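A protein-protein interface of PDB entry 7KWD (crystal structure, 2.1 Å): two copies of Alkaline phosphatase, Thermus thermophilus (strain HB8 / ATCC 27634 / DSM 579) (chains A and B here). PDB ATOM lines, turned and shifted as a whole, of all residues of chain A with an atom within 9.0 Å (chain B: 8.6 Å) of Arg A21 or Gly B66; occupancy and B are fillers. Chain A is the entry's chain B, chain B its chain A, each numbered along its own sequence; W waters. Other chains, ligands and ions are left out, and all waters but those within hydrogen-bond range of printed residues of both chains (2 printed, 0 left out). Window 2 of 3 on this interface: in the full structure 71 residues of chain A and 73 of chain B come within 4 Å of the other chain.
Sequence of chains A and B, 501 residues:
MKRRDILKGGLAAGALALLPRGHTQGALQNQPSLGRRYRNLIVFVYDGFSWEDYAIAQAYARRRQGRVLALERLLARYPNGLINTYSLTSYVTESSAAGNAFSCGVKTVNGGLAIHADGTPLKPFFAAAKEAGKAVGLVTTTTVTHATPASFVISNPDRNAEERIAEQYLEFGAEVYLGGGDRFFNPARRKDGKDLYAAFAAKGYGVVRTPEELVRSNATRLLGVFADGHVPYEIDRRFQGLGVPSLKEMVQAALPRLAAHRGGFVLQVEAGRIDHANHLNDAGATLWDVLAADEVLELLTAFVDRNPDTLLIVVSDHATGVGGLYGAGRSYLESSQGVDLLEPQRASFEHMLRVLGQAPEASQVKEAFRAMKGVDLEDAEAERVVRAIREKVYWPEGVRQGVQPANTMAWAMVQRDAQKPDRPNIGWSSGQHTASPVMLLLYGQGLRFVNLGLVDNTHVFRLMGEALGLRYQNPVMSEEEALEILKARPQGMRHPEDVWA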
ATOM      1  N   LEU A  18      25.042   0.695  15.059  1.00  0.00           N
ATOM      2  CA  LEU A  18      23.610   0.932  15.177  1.00  0.00           C
ATOM      3  C   LEU A  18      23.037   0.326  16.455  1.00  0.00           C
ATOM      4  O   LEU A  18      23.486  -0.720  16.939  1.00  0.00           O
ATOM      5  CB  LEU A  18      22.869   0.367  13.954  1.00  0.00           C
ATOM      6  CG  LEU A  18      22.702  -1.146  13.756  1.00  0.00           C
ATOM      7  CD1 LEU A  18      22.066  -1.420  12.382  1.00  0.00           C
ATOM      8  CD2 LEU A  18      24.005  -1.915  13.883  1.00  0.00           C
ATOM      9  N   LEU A  19      22.006   1.011  16.994  1.00  0.00           N
ATOM     10  CA  LEU A  19      21.374   0.669  18.252  1.00  0.00           C
ATOM     11  C   LEU A  19      20.369  -0.468  18.064  1.00  0.00           C
ATOM     12  O   LEU A  19      19.722  -0.574  17.022  1.00  0.00           O
ATOM     13  CB  LEU A  19      20.663   1.888  18.837  1.00  0.00           C
ATOM     14  CG  LEU A  19      21.539   2.980  19.473  1.00  0.00           C
ATOM     15  CD1 LEU A  19      20.867   4.353  19.391  1.00  0.00           C
ATOM     16  CD2 LEU A  19      21.839   2.634  20.913  1.00  0.00           C
ATOM     17  N   PRO A  20      20.209  -1.307  19.084  1.00  0.00           N
ATOM     18  CA  PRO A  20      19.289  -2.440  18.973  1.00  0.00           C
ATOM     19  C   PRO A  20      17.851  -2.008  18.766  1.00  0.00           C
ATOM     20  O   PRO A  20      17.426  -0.946  19.214  1.00  0.00           O
ATOM     21  CB  PRO A  20      19.458  -3.170  20.309  1.00  0.00           C
ATOM     22  CG  PRO A  20      19.976  -2.139  21.251  1.00  0.00           C
ATOM     23  CD  PRO A  20      20.778  -1.175  20.440  1.00  0.00           C
ATOM     24  N   ARG A  21      17.109  -2.868  18.081  1.00  0.00           N
ATOM     25  CA  ARG A  21      15.698  -2.638  17.831  1.00  0.00           C
ATOM     26  C   ARG A  21      14.943  -2.503  19.146  1.00  0.00           C
ATOM     27  O   ARG A  21      15.016  -3.369  20.014  1.00  0.00           O
ATOM     28  CB  ARG A  21      15.174  -3.804  16.989  1.00  0.00           C
ATOM     29  CG  ARG A  21      13.701  -3.789  16.665  1.00  0.00           C
ATOM     30  CD  ARG A  21      13.386  -4.760  15.507  1.00  0.00           C
ATOM     31  NE  ARG A  21      13.855  -6.136  15.719  1.00  0.00           N
ATOM     32  CZ  ARG A  21      13.328  -7.004  16.590  1.00  0.00           C
ATOM     33  NH1 ARG A  21      12.307  -6.658  17.374  1.00  0.00           N
ATOM     34  NH2 ARG A  21      13.839  -8.225  16.680  1.00  0.00           N
ATOM     35  N   GLY A  22      14.206  -1.403  19.286  1.00  0.00           N
ATOM     36  CA  GLY A  22      13.537  -1.081  20.532  1.00  0.00           C
ATOM     37  C   GLY A  22      14.308  -0.187  21.481  1.00  0.00           C
ATOM     38  O   GLY A  22      13.830   0.046  22.601  1.00  0.00           O
ATOM     39  N   HIS A  23      15.469   0.341  21.076  1.00  0.00           N
ATOM     40  CA  HIS A  23      16.301   1.095  22.010  1.00  0.00           C
ATOM     41  C   HIS A  23      15.572   2.288  22.631  1.00  0.00           C
ATOM     42  O   HIS A  23      15.893   2.688  23.754  1.00  0.00           O
ATOM     43  CB  HIS A  23      17.573   1.582  21.322  1.00  0.00           C
ATOM     44  CG  HIS A  23      17.337   2.463  20.135  1.00  0.00           C
ATOM     45  ND1 HIS A  23      17.347   3.839  20.216  1.00  0.00           N
ATOM     46  CD2 HIS A  23      17.137   2.164  18.829  1.00  0.00           C
ATOM     47  CE1 HIS A  23      17.150   4.350  19.012  1.00  0.00           C
ATOM     48  NE2 HIS A  23      17.006   3.356  18.157  1.00  0.00           N
ATOM     49  N   THR A  24      14.582   2.865  21.929  1.00  0.00           N
ATOM     50  CA  THR A  24      13.860   3.997  22.475  1.00  0.00           C
ATOM     51  C   THR A  24      13.036   3.610  23.691  1.00  0.00           C
ATOM     52  O   THR A  24      12.506   4.499  24.355  1.00  0.00           O
ATOM     53  CB  THR A  24      12.905   4.623  21.441  1.00  0.00           C
ATOM     54  OG1 THR A  24      11.896   3.663  21.083  1.00  0.00           O
ATOM     55  CG2 THR A  24      13.648   5.053  20.175  1.00  0.00           C
ATOM     56  N   GLN A  25      12.881   2.309  23.967  1.00  0.00           N
ATOM     57  CA  GLN A  25      12.098   1.852  25.105  1.00  0.00           C
ATOM     58  C   GLN A  25      12.955   1.150  26.152  1.00  0.00           C
ATOM     59  O   GLN A  25      12.417   0.586  27.104  1.00  0.00           O
ATOM     60  CB  GLN A  25      10.984   0.896  24.666  1.00  0.00           C
ATOM     61  CG  GLN A  25      10.255   1.276  23.413  1.00  0.00           C
ATOM     62  CD  GLN A  25       9.328   2.445  23.624  1.00  0.00           C
ATOM     63  OE1 GLN A  25       8.296   2.311  24.279  1.00  0.00           O
ATOM     64  NE2 GLN A  25       9.683   3.604  23.055  1.00  0.00           N
ATOM     65  N   GLY A  26      14.275   1.191  26.008  1.00  0.00           N
ATOM     66  CA  GLY A  26      15.160   0.484  26.910  1.00  0.00           C
ATOM     67  C   GLY A  26      15.382   1.240  28.205  1.00  0.00           C
ATOM     68  O   GLY A  26      14.919   2.367  28.402  1.00  0.00           O
ATOM     69  N   GLN B  58      18.566 -10.178  29.061  1.00  0.00           N
ATOM     70  CA  GLN B  58      18.653  -8.781  28.638  1.00  0.00           C
ATOM     71  C   GLN B  58      19.855  -8.559  27.722  1.00  0.00           C
ATOM     72  O   GLN B  58      19.738  -7.938  26.668  1.00  0.00           O
ATOM     73  CB  GLN B  58      18.756  -7.878  29.868  1.00  0.00           C
ATOM     74  CG  GLN B  58      18.837  -6.386  29.565  1.00  0.00           C
ATOM     75  CD  GLN B  58      19.009  -5.559  30.838  1.00  0.00           C
ATOM     76  OE1 GLN B  58      18.183  -4.702  31.154  1.00  0.00           O
ATOM     77  NE2 GLN B  58      20.087  -5.818  31.572  1.00  0.00           N
ATOM     78  N   ALA B  59      21.016  -9.089  28.122  1.00  0.00           N
ATOM     79  CA  ALA B  59      22.229  -8.931  27.340  1.00  0.00           C
ATOM     80  C   ALA B  59      22.144  -9.726  26.058  1.00  0.00           C
ATOM     81  O   ALA B  59      22.520  -9.235  24.989  1.00  0.00           O
ATOM     82  CB  ALA B  59      23.444  -9.373  28.157  1.00  0.00           C
ATOM     83  N   TYR B  60      21.633 -10.955  26.142  1.00  0.00           N
ATOM     84  CA  TYR B  60      21.580 -11.798  24.954  1.00  0.00           C
ATOM     85  C   TYR B  60      20.705 -11.168  23.874  1.00  0.00           C
ATOM     86  O   TYR B  60      21.057 -11.154  22.692  1.00  0.00           O
ATOM     87  CB  TYR B  60      21.070 -13.187  25.327  1.00  0.00           C
ATOM     88  CG  TYR B  60      21.190 -14.180  24.179  1.00  0.00           C
ATOM     89  CD1 TYR B  60      20.186 -14.310  23.256  1.00  0.00           C
ATOM     90  CD2 TYR B  60      22.342 -14.957  24.002  1.00  0.00           C
ATOM     91  CE1 TYR B  60      20.304 -15.181  22.191  1.00  0.00           C
ATOM     92  CE2 TYR B  60      22.447 -15.853  22.933  1.00  0.00           C
ATOM     93  CZ  TYR B  60      21.443 -15.953  22.040  1.00  0.00           C
ATOM     94  OH  TYR B  60      21.540 -16.816  20.962  1.00  0.00           O
ATOM     95  N   ALA B  61      19.528 -10.679  24.254  1.00  0.00           N
ATOM     96  CA  ALA B  61      18.652 -10.063  23.261  1.00  0.00           C
ATOM     97  C   ALA B  61      19.355  -8.893  22.562  1.00  0.00           C
ATOM     98  O   ALA B  61      19.320  -8.773  21.330  1.00  0.00           O
ATOM     99  CB  ALA B  61      17.348  -9.621  23.932  1.00  0.00           C
ATOM    100  N   ARG B  62      20.005  -8.022  23.332  1.00  0.00           N
ATOM    101  CA  ARG B  62      20.646  -6.861  22.729  1.00  0.00           C
ATOM    102  C   ARG B  62      21.848  -7.285  21.898  1.00  0.00           C
ATOM    103  O   ARG B  62      21.938  -6.972  20.705  1.00  0.00           O
ATOM    104  CB  ARG B  62      21.074  -5.868  23.802  1.00  0.00           C
ATOM    105  CG  ARG B  62      19.934  -4.965  24.284  1.00  0.00           C
ATOM    106  CD  ARG B  62      20.276  -4.331  25.670  1.00  0.00           C
ATOM    107  NE  ARG B  62      19.306  -3.298  26.044  1.00  0.00           N
ATOM    108  CZ  ARG B  62      19.318  -2.060  25.570  1.00  0.00           C
ATOM    109  NH1 ARG B  62      20.246  -1.648  24.699  1.00  0.00           N
ATOM    110  NH2 ARG B  62      18.376  -1.223  25.951  1.00  0.00           N
ATOM    111  N   ARG B  63      22.756  -8.057  22.513  1.00  0.00           N
ATOM    112  CA  ARG B  63      24.038  -8.369  21.899  1.00  0.00           C
ATOM    113  C   ARG B  63      23.926  -9.376  20.759  1.00  0.00           C
ATOM    114  O   ARG B  63      24.647  -9.261  19.760  1.00  0.00           O
ATOM    115  CB  ARG B  63      24.972  -8.898  22.979  1.00  0.00           C
ATOM    116  CG  ARG B  63      26.363  -9.152  22.511  1.00  0.00           C
ATOM    117  CD  ARG B  63      27.245  -9.472  23.696  1.00  0.00           C
ATOM    118  NE  ARG B  63      28.515 -10.046  23.289  1.00  0.00           N
ATOM    119  CZ  ARG B  63      29.676  -9.392  23.300  1.00  0.00           C
ATOM    120  NH1 ARG B  63      29.750  -8.127  23.703  1.00  0.00           N
ATOM    121  NH2 ARG B  63      30.783 -10.024  22.931  1.00  0.00           N
ATOM    122  N   ARG B  64      23.086 -10.406  20.898  1.00  0.00           N
ATOM    123  CA  ARG B  64      23.054 -11.461  19.894  1.00  0.00           C
ATOM    124  C   ARG B  64      21.837 -11.414  19.004  1.00  0.00           C
ATOM    125  O   ARG B  64      21.818 -12.083  17.961  1.00  0.00           O
ATOM    126  CB  ARG B  64      23.062 -12.860  20.525  1.00  0.00           C
ATOM    127  CG  ARG B  64      24.095 -13.117  21.583  1.00  0.00           C
ATOM    128  CD  ARG B  64      25.433 -12.639  21.162  1.00  0.00           C
ATOM    129  NE  ARG B  64      26.018 -13.475  20.120  1.00  0.00           N
ATOM    130  CZ  ARG B  64      26.737 -13.009  19.103  1.00  0.00           C
ATOM    131  NH1 ARG B  64      26.948 -11.699  18.951  1.00  0.00           N
ATOM    132  NH2 ARG B  64      27.248 -13.871  18.232  1.00  0.00           N
ATOM    133  N   GLN B  65      20.790 -10.721  19.411  1.00  0.00           N
ATOM    134  CA  GLN B  65      19.617 -10.589  18.560  1.00  0.00           C
ATOM    135  C   GLN B  65      19.369  -9.149  18.159  1.00  0.00           C
ATOM    136  O   GLN B  65      18.416  -8.892  17.437  1.00  0.00           O
ATOM    137  CB  GLN B  65      18.406 -11.183  19.276  1.00  0.00           C
ATOM    138  CG  GLN B  65      18.622 -12.672  19.656  1.00  0.00           C
ATOM    139  CD  GLN B  65      17.389 -13.331  20.260  1.00  0.00           C
ATOM    140  OE1 GLN B  65      16.534 -12.661  20.813  1.00  0.00           O
ATOM    141  NE2 GLN B  65      17.299 -14.654  20.142  1.00  0.00           N
ATOM    142  N   GLY B  66      20.220  -8.224  18.587  1.00  0.00           N
ATOM    143  CA  GLY B  66      20.034  -6.815  18.233  1.00  0.00           C
ATOM    144  C   GLY B  66      18.665  -6.272  18.563  1.00  0.00           C
ATOM    145  O   GLY B  66      18.122  -5.448  17.813  1.00  0.00           O
ATOM    146  N   ARG B  67      18.087  -6.703  19.687  1.00  0.00           N
ATOM    147  CA  ARG B  67      16.746  -6.265  20.099  1.00  0.00           C
ATOM    148  C   ARG B  67      16.739  -6.019  21.605  1.00  0.00           C
ATOM    149  O   ARG B  67      17.489  -6.649  22.363  1.00  0.00           O
ATOM    150  CB  ARG B  67      15.677  -7.324  19.756  1.00  0.00           C
ATOM    151  CG  ARG B  67      16.001  -8.663  20.481  1.00  0.00           C
ATOM    152  CD  ARG B  67      15.046  -9.817  20.243  1.00  0.00           C
ATOM    153  NE  ARG B  67      14.014  -9.770  21.256  1.00  0.00           N
ATOM    154  CZ  ARG B  67      13.692 -10.761  22.070  1.00  0.00           C
ATOM    155  NH1 ARG B  67      14.295 -11.942  22.020  1.00  0.00           N
ATOM    156  NH2 ARG B  67      12.712 -10.557  22.938  1.00  0.00           N
ATOM    157  N   VAL B  68      15.842  -5.143  22.039  1.00  0.00           N
ATOM    158  CA  VAL B  68      15.593  -4.934  23.460  1.00  0.00           C
ATOM    159  C   VAL B  68      14.520  -5.915  23.922  1.00  0.00           C
ATOM    160  O   VAL B  68      13.422  -5.935  23.378  1.00  0.00           O
ATOM    161  CB  VAL B  68      15.165  -3.496  23.744  1.00  0.00           C
ATOM    162  CG1 VAL B  68      14.908  -3.296  25.220  1.00  0.00           C
ATOM    163  CG2 VAL B  68      16.236  -2.556  23.222  1.00  0.00           C
ATOM    164  N   LEU B  69      14.843  -6.719  24.929  1.00  0.00           N
ATOM    165  CA  LEU B  69      13.896  -7.627  25.544  1.00  0.00           C
ATOM    166  C   LEU B  69      12.629  -6.905  25.978  1.00  0.00           C
ATOM    167  O   LEU B  69      12.688  -5.837  26.588  1.00  0.00           O
ATOM    168  CB  LEU B  69      14.607  -8.251  26.749  1.00  0.00           C
ATOM    169  CG  LEU B  69      14.119  -9.528  27.390  1.00  0.00           C
ATOM    170  CD1 LEU B  69      14.393 -10.699  26.503  1.00  0.00           C
ATOM    171  CD2 LEU B  69      14.834  -9.682  28.716  1.00  0.00           C
ATOM    172  N   ALA B  70      11.470  -7.492  25.667  1.00  0.00           N
ATOM    173  CA  ALA B  70      10.228  -6.853  26.068  1.00  0.00           C
ATOM    174  C   ALA B  70      10.178  -6.647  27.582  1.00  0.00           C
ATOM    175  O   ALA B  70       9.699  -5.618  28.062  1.00  0.00           O
ATOM    176  CB  ALA B  70       9.023  -7.655  25.597  1.00  0.00           C
ATOM    177  N   GLU B  72      12.636  -5.980  29.552  1.00  0.00           N
ATOM    178  CA  GLU B  72      13.389  -4.772  29.884  1.00  0.00           C
ATOM    179  C   GLU B  72      12.521  -3.525  29.660  1.00  0.00           C
ATOM    180  O   GLU B  72      12.485  -2.615  30.496  1.00  0.00           O
ATOM    181  CB  GLU B  72      14.684  -4.658  29.067  1.00  0.00           C
ATOM    182  CG  GLU B  72      15.435  -3.343  29.337  1.00  0.00           C
ATOM    183  CD  GLU B  72      16.677  -3.110  28.469  1.00  0.00           C
ATOM    184  OE1 GLU B  72      17.190  -4.075  27.882  1.00  0.00           O
ATOM    185  OE2 GLU B  72      17.123  -1.947  28.364  1.00  0.00           O
ATOM    186  N   ARG B  73      11.840  -3.454  28.511  1.00  0.00           N
ATOM    187  CA  ARG B  73      10.999  -2.284  28.229  1.00  0.00           C
ATOM    188  C   ARG B  73       9.952  -2.084  29.316  1.00  0.00           C
ATOM    189  O   ARG B  73       9.664  -0.941  29.696  1.00  0.00           O
ATOM    190  CB  ARG B  73      10.320  -2.433  26.873  1.00  0.00           C
ATOM    191  CG  ARG B  73      11.304  -2.727  25.745  1.00  0.00           C
ATOM    192  CD  ARG B  73      10.608  -2.887  24.350  1.00  0.00           C
ATOM    193  NE  ARG B  73      11.391  -3.683  23.385  1.00  0.00           N
ATOM    194  CZ  ARG B  73      11.236  -3.603  22.060  1.00  0.00           C
ATOM    195  NH1 ARG B  73      10.336  -2.774  21.543  1.00  0.00           N
ATOM    196  NH2 ARG B  73      11.992  -4.323  21.247  1.00  0.00           N
ATOM    197  N   ASP B 294       9.236 -14.043  26.880  1.00  0.00           N
ATOM    198  CA  ASP B 294       9.230 -12.686  26.352  1.00  0.00           C
ATOM    199  C   ASP B 294       8.282 -12.573  25.175  1.00  0.00           C
ATOM    200  O   ASP B 294       7.566 -11.573  25.034  1.00  0.00           O
ATOM    201  CB  ASP B 294      10.656 -12.270  25.973  1.00  0.00           C
ATOM    202  CG  ASP B 294      10.899 -10.785  26.151  1.00  0.00           C
ATOM    203  OD1 ASP B 294      10.868 -10.306  27.310  1.00  0.00           O
ATOM    204  OD2 ASP B 294      11.119 -10.103  25.141  1.00  0.00           O
ATOM    205  N   GLU B 298       4.781 -10.003  24.957  1.00  0.00           N
ATOM    206  CA  GLU B 298       4.388  -9.130  23.874  1.00  0.00           C
ATOM    207  C   GLU B 298       2.945  -9.367  23.530  1.00  0.00           C
ATOM    208  O   GLU B 298       2.186  -8.415  23.344  1.00  0.00           O
ATOM    209  CB  GLU B 298       5.297  -9.373  22.681  1.00  0.00           C
ATOM    210  CG  GLU B 298       6.670  -8.775  22.943  1.00  0.00           C
ATOM    211  CD  GLU B 298       7.620  -8.847  21.771  1.00  0.00           C
ATOM    212  OE1 GLU B 298       7.532  -9.825  20.998  1.00  0.00           O
ATOM    213  OE2 GLU B 298       8.477  -7.935  21.653  1.00  0.00           O
HETATM  214  O   HOH W   1      10.219   1.381  28.151  1.00  0.00           O
HETATM  215  O   HOH W   2      17.871   2.066  25.503  1.00  0.00           O
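No position is printed for both chains. Of the 13 pairs that touch across the chains among the printed residues, none has its exchanged pair printed and touching as well.
The guanidinium group of Arg B62 lies within salt-bridge range of the side-chain carboxylate of Glu B72, at 2.8 Å. The side-chain hydroxyl (OG1) of Thr A24 sits at hydrogen-bond distance from the side-chain amide nitrogen (NE2) of Gln A25, at 3.0 Å. N of Arg B62 sits at hydrogen-bond distance from O of Arg B67 (3.0 Å). The backbone carbonyl oxygen (O) of Ala B61 is in hydrogen-bond range of the backbone NH (N) of Gly B66. The backbone carbonyl oxygen of Ala B61 lies within hydrogen-bond range of the backbone NH of Arg B67, 2.9 Å away. The guanidinium group (NH1) of Arg B67 is in hydrogen-bond range of the side-chain amide oxygen (OE1) of Gln B65, 2.6 Å away.
Water W1 bridges the backbone carbonyl oxygen of Gln A25 and the backbone carbonyl oxygen of Arg B73. Water W2 lies within hydrogen-bond range of the backbone carbonyl oxygen (O) of His A23 (2.7 Å) and the guanidinium group (NH2) of Arg B62 (3.4 Å).
NH1 of Arg B62 touches CG of Pro A20, at 3.5 Å. Pro A20 touches Gly B66 (CA to O, 3.4 Å). Pro A20 touches Arg B67 (CB to N, 3.8 Å). CA of Arg B67 touches O of Arg A21 (3.4 Å). C of Gly A22 touches CG2 of Val B68 (3.5 Å). NH2 of Arg B73 touches CA of Gly A22, 3.7 Å away. N of His A23 touches CG2 of Val B68 (3.7 Å). Gln A25 touches Arg B73. Gly A26 touches Arg B62 (CA to NH2, 3.8 Å). OE2 of Glu B72 touches CA of Gly A26, 3.4 Å away.
The guanidinium group of Arg B73 lies within hydrogen-bond range of the backbone carbonyl oxygen of Arg A21 (3.4 Å). N of Val B68 is in hydrogen-bond range of O of Arg A21 (2.8 Å). O of Gly B66 lies within hydrogen-bond range of N of Arg A21, at 2.8 Å.
Printed residues of chain B within 4 Å of Pro A20: Arg B62 (3.5 Å), Gly B66 (3.4 Å) and Arg B67 (3.8 Å). Arg A21 touches just these residues of chain B: Gly B66, Arg B67, Val B68 and Arg B73. Of the printed residues of chain B, Gly A22 touches Val B68 (3.5 Å) and Arg B73 (3.7 Å). Printed residues of chain B within 4 Å of Gly A26: Arg B62 and Glu B72. Ala B59 touches none of the printed residues of chain A. Tyr B60 touches none of the printed residues of chain A. Printed residues of chain A within 4 Å of Gly B66: Pro A20 and Arg A21. Of the printed residues of chain A, Arg B67 touches Pro A20 and Arg A21. Printed residues of chain A within 4 Å of Val B68: Arg A21 (2.8 Å), Gly A22 (3.5 Å) and His A23 (3.7 Å). Printed residues of chain A within 4 Å of Arg B73: Arg A21, Gly A22 and Gln A25. The nearest residue of chain B that does not touch Arg A21 is Gln B65 (4.7 Å).
Of the 17 printed residues of chain B, 6 touch a printed residue of chain A. Of the 9 printed residues of chain A, 6 touch a printed residue of chain B.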
